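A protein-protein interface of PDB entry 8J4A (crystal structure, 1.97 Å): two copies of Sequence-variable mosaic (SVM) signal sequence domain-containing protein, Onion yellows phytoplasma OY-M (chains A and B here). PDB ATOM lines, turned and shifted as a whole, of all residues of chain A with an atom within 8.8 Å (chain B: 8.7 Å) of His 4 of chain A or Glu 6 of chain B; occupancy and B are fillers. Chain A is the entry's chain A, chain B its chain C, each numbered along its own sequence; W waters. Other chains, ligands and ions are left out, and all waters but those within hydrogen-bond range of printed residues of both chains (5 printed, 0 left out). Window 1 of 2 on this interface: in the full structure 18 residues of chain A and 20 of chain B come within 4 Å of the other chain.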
ATOM      1  N   ALA A   2     -15.746  20.017   9.339  1.00  0.00           N
ATOM      2  CA  ALA A   2     -16.223  21.390   9.222  1.00  0.00           C
ATOM      3  C   ALA A   2     -16.986  21.772  10.495  1.00  0.00           C
ATOM      4  O   ALA A   2     -17.458  20.898  11.216  1.00  0.00           O
ATOM      5  CB  ALA A   2     -17.109  21.544   7.971  1.00  0.00           C
ATOM      6  N   PRO A   3     -17.112  23.067  10.781  1.00  0.00           N
ATOM      7  CA  PRO A   3     -17.778  23.469  12.025  1.00  0.00           C
ATOM      8  C   PRO A   3     -19.293  23.326  11.949  1.00  0.00           C
ATOM      9  O   PRO A   3     -19.920  23.552  10.912  1.00  0.00           O
ATOM     10  CB  PRO A   3     -17.362  24.937  12.210  1.00  0.00           C
ATOM     11  CG  PRO A   3     -16.675  25.363  10.955  1.00  0.00           C
ATOM     12  CD  PRO A   3     -16.604  24.214  10.003  1.00  0.00           C
ATOM     13  N   HIS A   4     -19.877  22.922  13.066  1.00  0.00           N
ATOM     14  CA  HIS A   4     -21.330  22.922  13.212  1.00  0.00           C
ATOM     15  C   HIS A   4     -21.836  24.339  13.501  1.00  0.00           C
ATOM     16  O   HIS A   4     -21.264  25.057  14.332  1.00  0.00           O
ATOM     17  CB  HIS A   4     -21.735  21.970  14.340  1.00  0.00           C
ATOM     18  CG  HIS A   4     -23.188  22.036  14.686  1.00  0.00           C
ATOM     19  ND1 HIS A   4     -23.681  22.862  15.678  1.00  0.00           N
ATOM     20  CD2 HIS A   4     -24.258  21.384  14.166  1.00  0.00           C
ATOM     21  CE1 HIS A   4     -24.991  22.707  15.755  1.00  0.00           C
ATOM     22  NE2 HIS A   4     -25.366  21.818  14.850  1.00  0.00           N
ATOM     23  N   GLU A   5     -22.910  24.744  12.828  1.00  0.00           N
ATOM     24  CA  GLU A   5     -23.508  26.054  13.062  1.00  0.00           C
ATOM     25  C   GLU A   5     -25.017  25.918  13.164  1.00  0.00           C
ATOM     26  O   GLU A   5     -25.644  25.303  12.297  1.00  0.00           O
ATOM     27  CB  GLU A   5     -23.165  27.058  11.945  1.00  0.00           C
ATOM     28  CG  GLU A   5     -21.802  26.857  11.284  1.00  0.00           C
ATOM     29  CD  GLU A   5     -21.633  27.659   9.986  1.00  0.00           C
ATOM     30  OE1 GLU A   5     -21.454  28.897  10.064  1.00  0.00           O
ATOM     31  OE2 GLU A   5     -21.680  27.048   8.891  1.00  0.00           O
ATOM     32  N   GLU A   6     -25.593  26.482  14.219  1.00  0.00           N
ATOM     33  CA  GLU A   6     -27.040  26.644  14.333  1.00  0.00           C
ATOM     34  C   GLU A   6     -27.327  28.090  14.720  1.00  0.00           C
ATOM     35  O   GLU A   6     -26.649  28.657  15.591  1.00  0.00           O
ATOM     36  CB  GLU A   6     -27.651  25.688  15.373  1.00  0.00           C
ATOM     37  CG  GLU A   6     -29.184  25.830  15.492  1.00  0.00           C
ATOM     38  CD  GLU A   6     -29.839  24.803  16.405  1.00  0.00           C
ATOM     39  OE1 GLU A   6     -29.128  23.966  17.010  1.00  0.00           O
ATOM     40  OE2 GLU A   6     -31.091  24.838  16.533  1.00  0.00           O
ATOM     41  N   ARG A   7     -28.330  28.689  14.084  1.00  0.00           N
ATOM     42  CA  ARG A   7     -28.548  30.104  14.311  1.00  0.00           C
ATOM     43  C   ARG A   7     -29.940  30.510  13.856  1.00  0.00           C
ATOM     44  O   ARG A   7     -30.595  29.828  13.055  1.00  0.00           O
ATOM     45  CB  ARG A   7     -27.480  30.957  13.614  1.00  0.00           C
ATOM     46  CG  ARG A   7     -27.663  31.129  12.105  1.00  0.00           C
ATOM     47  CD  ARG A   7     -26.707  32.195  11.562  1.00  0.00           C
ATOM     48  NE  ARG A   7     -25.441  32.213  12.301  1.00  0.00           N
ATOM     49  CZ  ARG A   7     -25.060  33.185  13.132  1.00  0.00           C
ATOM     50  NH1 ARG A   7     -25.853  34.233  13.353  1.00  0.00           N
ATOM     51  NH2 ARG A   7     -23.895  33.103  13.772  1.00  0.00           N
ATOM     52  N   VAL A   8     -30.399  31.615  14.433  1.00  0.00           N
ATOM     53  CA  VAL A   8     -31.608  32.307  14.003  1.00  0.00           C
ATOM     54  C   VAL A   8     -31.200  33.760  13.844  1.00  0.00           C
ATOM     55  O   VAL A   8     -30.954  34.450  14.845  1.00  0.00           O
ATOM     56  CB  VAL A   8     -32.761  32.163  15.001  1.00  0.00           C
ATOM     57  CG1 VAL A   8     -33.977  32.972  14.534  1.00  0.00           C
ATOM     58  CG2 VAL A   8     -33.138  30.688  15.163  1.00  0.00           C
ATOM     59  N   ARG A  12     -26.778  33.200  17.872  1.00  0.00           N
ATOM     60  CA  ARG A  12     -26.127  31.904  17.850  1.00  0.00           C
ATOM     61  C   ARG A  12     -26.877  30.957  18.779  1.00  0.00           C
ATOM     62  O   ARG A  12     -27.238  31.335  19.900  1.00  0.00           O
ATOM     63  CB  ARG A  12     -24.661  32.040  18.273  1.00  0.00           C
ATOM     64  CG  ARG A  12     -23.901  30.723  18.337  1.00  0.00           C
ATOM     65  CD  ARG A  12     -22.513  30.909  18.955  1.00  0.00           C
ATOM     66  NE  ARG A  12     -21.624  31.678  18.094  1.00  0.00           N
ATOM     67  CZ  ARG A  12     -21.236  32.918  18.351  1.00  0.00           C
ATOM     68  NH1 ARG A  12     -21.668  33.536  19.455  1.00  0.00           N
ATOM     69  NH2 ARG A  12     -20.415  33.537  17.509  1.00  0.00           N
ATOM     70  N   ILE A  13     -27.125  29.733  18.314  1.00  0.00           N
ATOM     71  CA  ILE A  13     -27.720  28.696  19.147  1.00  0.00           C
ATOM     72  C   ILE A  13     -26.613  27.742  19.581  1.00  0.00           C
ATOM     73  O   ILE A  13     -25.956  27.106  18.744  1.00  0.00           O
ATOM     74  CB  ILE A  13     -28.860  27.975  18.413  1.00  0.00           C
ATOM     75  CG1 ILE A  13     -30.029  28.945  18.266  1.00  0.00           C
ATOM     76  CG2 ILE A  13     -29.308  26.722  19.172  1.00  0.00           C
ATOM     77  CD1 ILE A  13     -31.128  28.413  17.372  1.00  0.00           C
ATOM     78  N   VAL A  14     -26.406  27.654  20.898  1.00  0.00           N
ATOM     79  CA  VAL A  14     -25.326  26.893  21.509  1.00  0.00           C
ATOM     80  C   VAL A  14     -25.943  25.733  22.288  1.00  0.00           C
ATOM     81  O   VAL A  14     -26.589  25.934  23.322  1.00  0.00           O
ATOM     82  CB  VAL A  14     -24.456  27.765  22.429  1.00  0.00           C
ATOM     83  CG1 VAL A  14     -23.236  26.987  22.878  1.00  0.00           C
ATOM     84  CG2 VAL A  14     -24.026  29.065  21.720  1.00  0.00           C
ATOM     85  N   ASN A  15     -25.734  24.518  21.798  1.00  0.00           N
ATOM     86  CA  ASN A  15     -26.257  23.309  22.414  1.00  0.00           C
ATOM     87  C   ASN A  15     -25.158  22.751  23.299  1.00  0.00           C
ATOM     88  O   ASN A  15     -24.030  22.553  22.836  1.00  0.00           O
ATOM     89  CB  ASN A  15     -26.686  22.285  21.355  1.00  0.00           C
ATOM     90  CG  ASN A  15     -27.886  22.751  20.538  1.00  0.00           C
ATOM     91  OD1 ASN A  15     -29.025  22.660  20.993  1.00  0.00           O
ATOM     92  ND2 ASN A  15     -27.633  23.271  19.330  1.00  0.00           N
ATOM     93  N   LYS A  86     -36.992  29.479  19.803  1.00  0.00           N
ATOM     94  CA  LYS A  86     -35.874  29.793  18.927  1.00  0.00           C
ATOM     95  C   LYS A  86     -36.119  31.071  18.150  1.00  0.00           C
ATOM     96  O   LYS A  86     -35.161  31.708  17.705  1.00  0.00           O
ATOM     97  CB  LYS A  86     -35.569  28.628  17.990  1.00  0.00           C
ATOM     98  CG  LYS A  86     -34.786  27.530  18.688  1.00  0.00           C
ATOM     99  CD  LYS A  86     -34.680  26.283  17.830  1.00  0.00           C
ATOM    100  CE  LYS A  86     -33.935  25.169  18.556  1.00  0.00           C
ATOM    101  NZ  LYS A  86     -33.903  23.908  17.753  1.00  0.00           N
ATOM    102  N   PRO B   3     -35.024  33.187   9.562  1.00  0.00           N
ATOM    103  CA  PRO B   3     -34.975  31.746   9.286  1.00  0.00           C
ATOM    104  C   PRO B   3     -34.067  31.055  10.285  1.00  0.00           C
ATOM    105  O   PRO B   3     -32.958  31.517  10.559  1.00  0.00           O
ATOM    106  CB  PRO B   3     -34.398  31.663   7.866  1.00  0.00           C
ATOM    107  CG  PRO B   3     -34.319  33.058   7.360  1.00  0.00           C
ATOM    108  CD  PRO B   3     -34.275  33.944   8.540  1.00  0.00           C
ATOM    109  N   HIS B   4     -34.541  29.947  10.833  1.00  0.00           N
ATOM    110  CA  HIS B   4     -33.632  29.051  11.525  1.00  0.00           C
ATOM    111  C   HIS B   4     -32.758  28.323  10.518  1.00  0.00           C
ATOM    112  O   HIS B   4     -33.220  27.925   9.441  1.00  0.00           O
ATOM    113  CB  HIS B   4     -34.406  28.043  12.359  1.00  0.00           C
ATOM    114  CG  HIS B   4     -33.576  26.893  12.844  1.00  0.00           C
ATOM    115  ND1 HIS B   4     -33.353  25.766  12.081  1.00  0.00           N
ATOM    116  CD2 HIS B   4     -32.946  26.681  14.025  1.00  0.00           C
ATOM    117  CE1 HIS B   4     -32.618  24.910  12.771  1.00  0.00           C
ATOM    118  NE2 HIS B   4     -32.356  25.440  13.955  1.00  0.00           N
ATOM    119  N   GLU B   5     -31.493  28.129  10.877  1.00  0.00           N
ATOM    120  CA  GLU B   5     -30.610  27.345  10.023  1.00  0.00           C
ATOM    121  C   GLU B   5     -29.636  26.530  10.857  1.00  0.00           C
ATOM    122  O   GLU B   5     -29.018  27.070  11.787  1.00  0.00           O
ATOM    123  CB  GLU B   5     -29.867  28.265   9.044  1.00  0.00           C
ATOM    124  CG  GLU B   5     -29.578  27.629   7.655  1.00  0.00           C
ATOM    125  CD  GLU B   5     -30.843  26.977   6.952  1.00  0.00           C
ATOM    126  OE1 GLU B   5     -30.720  25.908   6.352  1.00  0.00           O
ATOM    127  OE2 GLU B   5     -31.926  27.576   7.023  1.00  0.00           O
ATOM    128  N   GLU B   6     -29.520  25.237  10.532  1.00  0.00           N
ATOM    129  CA  GLU B   6     -28.505  24.354  11.110  1.00  0.00           C
ATOM    130  C   GLU B   6     -27.707  23.724   9.976  1.00  0.00           C
ATOM    131  O   GLU B   6     -28.286  23.253   8.992  1.00  0.00           O
ATOM    132  CB  GLU B   6     -29.121  23.272  12.005  1.00  0.00           C
ATOM    133  CG  GLU B   6     -28.070  22.542  12.864  1.00  0.00           C
ATOM    134  CD  GLU B   6     -28.634  21.435  13.763  1.00  0.00           C
ATOM    135  OE1 GLU B   6     -29.872  21.326  13.893  1.00  0.00           O
ATOM    136  OE2 GLU B   6     -27.818  20.681  14.361  1.00  0.00           O
ATOM    137  N   ARG B   7     -26.387  23.717  10.120  1.00  0.00           N
ATOM    138  CA  ARG B   7     -25.477  23.440   9.012  1.00  0.00           C
ATOM    139  C   ARG B   7     -24.201  22.810   9.540  1.00  0.00           C
ATOM    140  O   ARG B   7     -23.742  23.136  10.639  1.00  0.00           O
ATOM    141  CB  ARG B   7     -25.102  24.722   8.256  1.00  0.00           C
ATOM    142  CG  ARG B   7     -26.128  25.190   7.249  1.00  0.00           C
ATOM    143  CD  ARG B   7     -25.527  25.292   5.866  1.00  0.00           C
ATOM    144  NE  ARG B   7     -26.500  25.052   4.803  1.00  0.00           N
ATOM    145  CZ  ARG B   7     -26.149  24.706   3.571  1.00  0.00           C
ATOM    146  NH1 ARG B   7     -24.863  24.569   3.292  1.00  0.00           N
ATOM    147  NH2 ARG B   7     -27.061  24.499   2.623  1.00  0.00           N
ATOM    148  N   VAL B   8     -23.621  21.920   8.741  1.00  0.00           N
ATOM    149  CA  VAL B   8     -22.230  21.503   8.886  1.00  0.00           C
ATOM    150  C   VAL B   8     -21.618  21.638   7.496  1.00  0.00           C
ATOM    151  O   VAL B   8     -21.816  20.769   6.634  1.00  0.00           O
ATOM    152  CB  VAL B   8     -22.079  20.079   9.425  1.00  0.00           C
ATOM    153  CG1 VAL B   8     -20.609  19.618   9.322  1.00  0.00           C
ATOM    154  CG2 VAL B   8     -22.583  19.988  10.857  1.00  0.00           C
ATOM    155  N   GLY B   9     -20.900  22.739   7.266  1.00  0.00           N
ATOM    156  CA  GLY B   9     -20.347  23.012   5.948  1.00  0.00           C
ATOM    157  C   GLY B   9     -21.456  23.221   4.939  1.00  0.00           C
ATOM    158  O   GLY B   9     -22.410  23.973   5.168  1.00  0.00           O
ATOM    159  N   ASP B  10     -21.356  22.523   3.814  1.00  0.00           N
ATOM    160  CA  ASP B  10     -22.386  22.612   2.798  1.00  0.00           C
ATOM    161  C   ASP B  10     -23.519  21.629   3.020  1.00  0.00           C
ATOM    162  O   ASP B  10     -24.371  21.487   2.141  1.00  0.00           O
ATOM    163  CB  ASP B  10     -21.782  22.436   1.405  1.00  0.00           C
ATOM    164  CG  ASP B  10     -20.762  23.507   1.084  1.00  0.00           C
ATOM    165  OD1 ASP B  10     -20.596  23.845  -0.110  1.00  0.00           O
ATOM    166  OD2 ASP B  10     -20.128  24.022   2.032  1.00  0.00           O
ATOM    167  N   MET B  11     -23.570  20.973   4.175  1.00  0.00           N
ATOM    168  CA  MET B  11     -24.664  20.071   4.495  1.00  0.00           C
ATOM    169  C   MET B  11     -25.668  20.771   5.403  1.00  0.00           C
ATOM    170  O   MET B  11     -25.317  21.242   6.497  1.00  0.00           O
ATOM    171  CB  MET B  11     -24.158  18.788   5.147  1.00  0.00           C
ATOM    172  CG  MET B  11     -25.303  17.808   5.444  1.00  0.00           C
ATOM    173  SD  MET B  11     -24.788  16.257   6.187  1.00  0.00           S
ATOM    174  CE  MET B  11     -24.352  16.797   7.823  1.00  0.00           C
ATOM    175  N   ARG B  12     -26.914  20.808   4.953  1.00  0.00           N
ATOM    176  CA  ARG B  12     -28.022  21.345   5.719  1.00  0.00           C
ATOM    177  C   ARG B  12     -28.581  20.288   6.670  1.00  0.00           C
ATOM    178  O   ARG B  12     -28.704  19.116   6.313  1.00  0.00           O
ATOM    179  CB  ARG B  12     -29.108  21.822   4.762  1.00  0.00           C
ATOM    180  CG  ARG B  12     -30.315  22.340   5.420  1.00  0.00           C
ATOM    181  CD  ARG B  12     -31.448  22.419   4.430  1.00  0.00           C
ATOM    182  NE  ARG B  12     -31.301  23.606   3.610  1.00  0.00           N
ATOM    183  CZ  ARG B  12     -30.952  23.585   2.334  1.00  0.00           C
ATOM    184  NH1 ARG B  12     -30.740  22.418   1.726  1.00  0.00           N
ATOM    185  NH2 ARG B  12     -30.833  24.732   1.666  1.00  0.00           N
ATOM    186  N   ILE B  13     -28.907  20.705   7.888  1.00  0.00           N
ATOM    187  CA  ILE B  13     -29.503  19.825   8.892  1.00  0.00           C
ATOM    188  C   ILE B  13     -30.981  20.178   8.998  1.00  0.00           C
ATOM    189  O   ILE B  13     -31.332  21.327   9.295  1.00  0.00           O
ATOM    190  CB  ILE B  13     -28.800  19.956  10.247  1.00  0.00           C
ATOM    191  CG1 ILE B  13     -27.302  19.825  10.058  1.00  0.00           C
ATOM    192  CG2 ILE B  13     -29.321  18.903  11.244  1.00  0.00           C
ATOM    193  CD1 ILE B  13     -26.878  18.433   9.786  1.00  0.00           C
ATOM    194  N   VAL B  14     -31.844  19.191   8.766  1.00  0.00           N
ATOM    195  CA  VAL B  14     -33.285  19.375   8.655  1.00  0.00           C
ATOM    196  C   VAL B  14     -33.932  18.557   9.772  1.00  0.00           C
ATOM    197  O   VAL B  14     -34.042  17.330   9.678  1.00  0.00           O
ATOM    198  CB  VAL B  14     -33.821  18.947   7.277  1.00  0.00           C
ATOM    199  CG1 VAL B  14     -35.280  19.335   7.133  1.00  0.00           C
ATOM    200  CG2 VAL B  14     -32.994  19.567   6.142  1.00  0.00           C
ATOM    201  N   ASN B  15     -34.392  19.229  10.817  1.00  0.00           N
ATOM    202  CA  ASN B  15     -35.091  18.572  11.912  1.00  0.00           C
ATOM    203  C   ASN B  15     -36.579  18.475  11.601  1.00  0.00           C
ATOM    204  O   ASN B  15     -37.206  19.470  11.231  1.00  0.00           O
ATOM    205  CB  ASN B  15     -34.829  19.346  13.206  1.00  0.00           C
ATOM    206  CG  ASN B  15     -33.335  19.408  13.528  1.00  0.00           C
ATOM    207  OD1 ASN B  15     -32.765  18.439  14.008  1.00  0.00           O
ATOM    208  ND2 ASN B  15     -32.691  20.519  13.192  1.00  0.00           N
ATOM    209  N   ILE B  16     -37.127  17.270  11.715  1.00  0.00           N
ATOM    210  CA  ILE B  16     -38.522  16.983  11.381  1.00  0.00           C
ATOM    211  C   ILE B  16     -39.139  16.221  12.540  1.00  0.00           C
ATOM    212  O   ILE B  16     -38.564  15.228  12.993  1.00  0.00           O
ATOM    213  CB  ILE B  16     -38.625  16.140  10.097  1.00  0.00           C
ATOM    214  CG1 ILE B  16     -37.912  16.822   8.942  1.00  0.00           C
ATOM    215  CG2 ILE B  16     -40.075  15.820   9.771  1.00  0.00           C
ATOM    216  CD1 ILE B  16     -38.024  16.035   7.647  1.00  0.00           C
ATOM    217  N   LEU B  82     -25.500  10.795  17.827  1.00  0.00           N
ATOM    218  CA  LEU B  82     -26.127  11.730  16.894  1.00  0.00           C
ATOM    219  C   LEU B  82     -25.209  12.904  16.576  1.00  0.00           C
ATOM    220  O   LEU B  82     -25.160  13.378  15.433  1.00  0.00           O
ATOM    221  CB  LEU B  82     -27.446  12.230  17.459  1.00  0.00           C
ATOM    222  CG  LEU B  82     -28.135  13.285  16.597  1.00  0.00           C
ATOM    223  CD1 LEU B  82     -28.596  12.640  15.275  1.00  0.00           C
ATOM    224  CD2 LEU B  82     -29.296  13.809  17.360  1.00  0.00           C
ATOM    225  N   GLU B  83     -24.463  13.377  17.571  1.00  0.00           N
ATOM    226  CA  GLU B  83     -23.555  14.490  17.343  1.00  0.00           C
ATOM    227  C   GLU B  83     -22.436  14.129  16.373  1.00  0.00           C
ATOM    228  O   GLU B  83     -22.060  14.943  15.523  1.00  0.00           O
ATOM    229  CB  GLU B  83     -22.958  14.948  18.670  1.00  0.00           C
ATOM    230  CG  GLU B  83     -23.715  16.036  19.343  1.00  0.00           C
ATOM    231  CD  GLU B  83     -23.048  16.411  20.646  1.00  0.00           C
ATOM    232  OE1 GLU B  83     -21.918  16.963  20.590  1.00  0.00           O
ATOM    233  OE2 GLU B  83     -23.631  16.117  21.720  1.00  0.00           O
ATOM    234  N   LYS B  86     -23.448  14.064  12.739  1.00  0.00           N
ATOM    235  CA  LYS B  86     -23.510  15.370  12.082  1.00  0.00           C
ATOM    236  C   LYS B  86     -22.231  15.692  11.329  1.00  0.00           C
ATOM    237  O   LYS B  86     -22.263  16.469  10.361  1.00  0.00           O
ATOM    238  CB  LYS B  86     -23.815  16.480  13.097  1.00  0.00           C
ATOM    239  CG  LYS B  86     -25.165  16.309  13.824  1.00  0.00           C
ATOM    240  CD  LYS B  86     -25.600  17.592  14.523  1.00  0.00           C
ATOM    241  CE  LYS B  86     -26.812  17.368  15.403  1.00  0.00           C
ATOM    242  NZ  LYS B  86     -27.094  18.539  16.302  1.00  0.00           N
ATOM    243  N   GLN B  87     -21.121  15.083  11.709  1.00  0.00           N
ATOM    244  CA  GLN B  87     -19.862  15.269  10.995  1.00  0.00           C
ATOM    245  C   GLN B  87     -19.647  14.234   9.894  1.00  0.00           C
ATOM    246  O   GLN B  87     -18.577  14.212   9.270  1.00  0.00           O
ATOM    247  CB  GLN B  87     -18.696  15.227  11.982  1.00  0.00           C
ATOM    248  CG  GLN B  87     -18.629  16.446  12.914  1.00  0.00           C
ATOM    249  CD  GLN B  87     -18.419  17.757  12.169  1.00  0.00           C
ATOM    250  OE1 GLN B  87     -17.740  17.804  11.137  1.00  0.00           O
ATOM    251  NE2 GLN B  87     -19.000  18.831  12.689  1.00  0.00           N
ATOM    252  N   LYS B  93     -25.889  16.509   0.962  1.00  0.00           N
ATOM    253  CA  LYS B  93     -26.294  17.900   1.055  1.00  0.00           C
ATOM    254  C   LYS B  93     -27.359  18.134   2.118  1.00  0.00           C
ATOM    255  O   LYS B  93     -27.602  19.284   2.484  1.00  0.00           O
ATOM    256  CB  LYS B  93     -26.822  18.385  -0.300  1.00  0.00           C
ATOM    257  CG  LYS B  93     -25.816  18.262  -1.437  1.00  0.00           C
ATOM    258  CD  LYS B  93     -25.007  19.534  -1.586  1.00  0.00           C
ATOM    259  CE  LYS B  93     -23.552  19.238  -1.928  1.00  0.00           C
ATOM    260  NZ  LYS B  93     -22.887  20.444  -2.521  1.00  0.00           N
ATOM    261  N   ASN B  94     -28.027  17.078   2.583  1.00  0.00           N
ATOM    262  CA  ASN B  94     -29.044  17.208   3.613  1.00  0.00           C
ATOM    263  C   ASN B  94     -28.943  16.031   4.559  1.00  0.00           C
ATOM    264  O   ASN B  94     -28.807  14.878   4.126  1.00  0.00           O
ATOM    265  CB  ASN B  94     -30.456  17.269   3.036  1.00  0.00           C
ATOM    266  CG  ASN B  94     -30.694  18.509   2.214  1.00  0.00           C
ATOM    267  OD1 ASN B  94     -31.051  19.558   2.748  1.00  0.00           O
ATOM    268  ND2 ASN B  94     -30.495  18.402   0.903  1.00  0.00           N
ATOM    269  N   MET B  95     -28.985  16.334   5.850  1.00  0.00           N
ATOM    270  CA  MET B  95     -29.082  15.330   6.898  1.00  0.00           C
ATOM    271  C   MET B  95     -30.426  15.534   7.589  1.00  0.00           C
ATOM    272  O   MET B  95     -30.630  16.536   8.287  1.00  0.00           O
ATOM    273  CB  MET B  95     -27.919  15.431   7.880  1.00  0.00           C
ATOM    274  CG  MET B  95     -28.066  14.524   9.120  1.00  0.00           C
ATOM    275  SD  MET B  95     -26.911  15.013  10.433  1.00  0.00           S
ATOM    276  CE  MET B  95     -27.164  13.667  11.595  1.00  0.00           C
ATOM    277  N   ILE B  97     -33.142  14.636  10.332  1.00  0.00           N
ATOM    278  CA  ILE B  97     -33.186  14.085  11.684  1.00  0.00           C
ATOM    279  C   ILE B  97     -34.642  14.050  12.111  1.00  0.00           C
ATOM    280  O   ILE B  97     -35.286  15.105  12.235  1.00  0.00           O
ATOM    281  CB  ILE B  97     -32.340  14.904  12.673  1.00  0.00           C
ATOM    282  CG1 ILE B  97     -30.905  15.026  12.154  1.00  0.00           C
ATOM    283  CG2 ILE B  97     -32.378  14.259  14.054  1.00  0.00           C
ATOM    284  CD1 ILE B  97     -29.994  15.856  13.024  1.00  0.00           C
ATOM    285  N   TRP B  99     -37.602  13.336  14.709  1.00  0.00           N
ATOM    286  CA  TRP B  99     -37.817  13.426  16.143  1.00  0.00           C
ATOM    287  C   TRP B  99     -39.257  13.055  16.476  1.00  0.00           C
ATOM    288  O   TRP B  99     -40.181  13.341  15.714  1.00  0.00           O
ATOM    289  CB  TRP B  99     -37.542  14.844  16.647  1.00  0.00           C
ATOM    290  CG  TRP B  99     -36.161  15.352  16.447  1.00  0.00           C
ATOM    291  CD1 TRP B  99     -35.731  16.205  15.458  1.00  0.00           C
ATOM    292  CD2 TRP B  99     -35.019  15.085  17.271  1.00  0.00           C
ATOM    293  NE1 TRP B  99     -34.388  16.467  15.619  1.00  0.00           N
ATOM    294  CE2 TRP B  99     -33.931  15.800  16.726  1.00  0.00           C
ATOM    295  CE3 TRP B  99     -34.807  14.305  18.412  1.00  0.00           C
ATOM    296  CZ2 TRP B  99     -32.660  15.760  17.288  1.00  0.00           C
ATOM    297  CZ3 TRP B  99     -33.549  14.269  18.958  1.00  0.00           C
ATOM    298  CH2 TRP B  99     -32.490  14.987  18.400  1.00  0.00           C
HETATM  299  O   HOH W   1     -22.186  27.011   5.811  1.00  0.00           O
HETATM  300  O   HOH W   2     -28.508  20.789  17.349  1.00  0.00           O
HETATM  301  O   HOH W   3     -19.946  25.015   8.630  1.00  0.00           O
HETATM  302  O   HOH W   4     -24.077  19.069  22.859  1.00  0.00           O
HETATM  303  O   HOH W   5     -31.782  21.965  15.694  1.00  0.00           O
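The backbone carbonyl oxygen (O) of Ala 2 of chain A is in hydrogen-bond range of the side-chain amide nitrogen (NE2) of Gln 87 of chain B (3.0 Å).
NE2 of His 4 of chain A is in hydrogen-bond range of OE2 of Glu 6 of chain B.
The backbone NH (N) of Arg 7 of chain B lies within hydrogen-bond range of the backbone carbonyl oxygen (O) of Glu 5 of chain A (2.8 Å).
OE2 of Glu 6 of chain A sits at hydrogen-bond distance from NE2 of His 4 of chain B (2.9 Å).
The backbone NH (N) of Arg 7 of chain A lies within hydrogen-bond range of the backbone carbonyl oxygen (O) of Glu 5 of chain B, at 2.9 Å.
Printed residues of chain B within 4 Å of His 4 of chain A: Glu 6, Arg 7, Val 8 and Lys 86.
Glu 6 of chain B touches just these residues of chain A: His 4 and Glu 5.
Of the printed residues of chain A, Gly 9 of chain B touches Pro 3 (3.9 Å).
Of the printed residues of chain A, Lys 86 of chain B touches His 4.
Of the printed residues of chain B, Glu 6 of chain A touches His 4 (2.9 Å) and Glu 5 (3.3 Å).
The nearest printed residue of chain B that does not touch His 4 of chain A is Gln 87 of chain B (4.2 Å).
The nearest residue of chain A that does not touch Glu 6 of chain B is Glu 6 of chain A (4.05 Å).
The nearest printed residue of chain A that does not touch His 4 of chain B is Val 8 of chain A (4.02 Å).
Printed residues of chain B that touch a printed residue of chain A: Pro 3, His 4, Glu 5, Glu 6, Arg 7, Val 8, Gly 9, Lys 86 and Gln 87.
Hydrophobic or aromatic side chains of chain B within 4 Å of the printed part of chain A: His 4 and Val 8.
Hydrophobic or aromatic side chains of chain A that line the printed part of chain B: His 4.
Among the printed residues, 18 pairs touch across the chains.
Water W5 lies within hydrogen-bond range of the side-chain carboxylate of Glu 6 of chain B, the side-chain amide nitrogen of Asn 15 of chain B and the side-chain carboxylate of Glu 6 of chain A.
Water W2 lies within hydrogen-bond range of NZ of Lys 86 of chain B, OE2 of Glu 6 of chain B, OE1 of Glu 6 of chain A and ND2 of Asn 15 of chain A.
Water W4 lies within hydrogen-bond range of OE2 of Glu 83 of chain B and O of Asn 15 of chain A.
His 4 of chain A touches Val 8 of chain B, but with the chains exchanged Val 8 of chain A does not touch His 4 of chain B (4.02 Å).
Glu 5 of chain B touches its own counterpart, Glu 5 of chain A.
Glu 5 of chain A touches Glu 6 of chain B, and with the chains exchanged Glu 6 of chain A touches Glu 5 of chain B.
Glu 5 of chain A touches Arg 7 of chain B, and with the chains exchanged Arg 7 of chain A touches Glu 5 of chain B.
Val 8 of chain B touches Ala 2 of chain A (CG1 to O, 3.9 Å).
Gly 9 of chain B touches Pro 3 of chain A (N to O, 3.9 Å).
His 4 of chain A touches Val 8 of chain B (CD2 to CG2, 3.96 Å).
Lys 86 of chain B touches His 4 of chain A.
Glu 5 of chain B touches Glu 6 of chain A.
Pro 3 of chain B touches Arg 7 of chain A (O to O, 3.8 Å).
O of Arg 7 of chain A touches CA of His 4 of chain B, at 3.5 Å.
OE1 of Glu 6 of chain A lies within hydrogen-bond range of ND2 of Asn 15 of chain A.
OE1 of Glu 6 of chain B sits at hydrogen-bond distance from ND2 of Asn 15 of chain B (3.0 Å).
The guanidinium group of Arg 7 of chain B is in hydrogen-bond range of the backbone carbonyl oxygen of Gly 9 of chain B (3.1 Å).
The guanidinium group (NH1) of Arg 7 of chain B sits close to the backbone carbonyl oxygen (O) of Asp 10 of chain B (3.3 Å).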
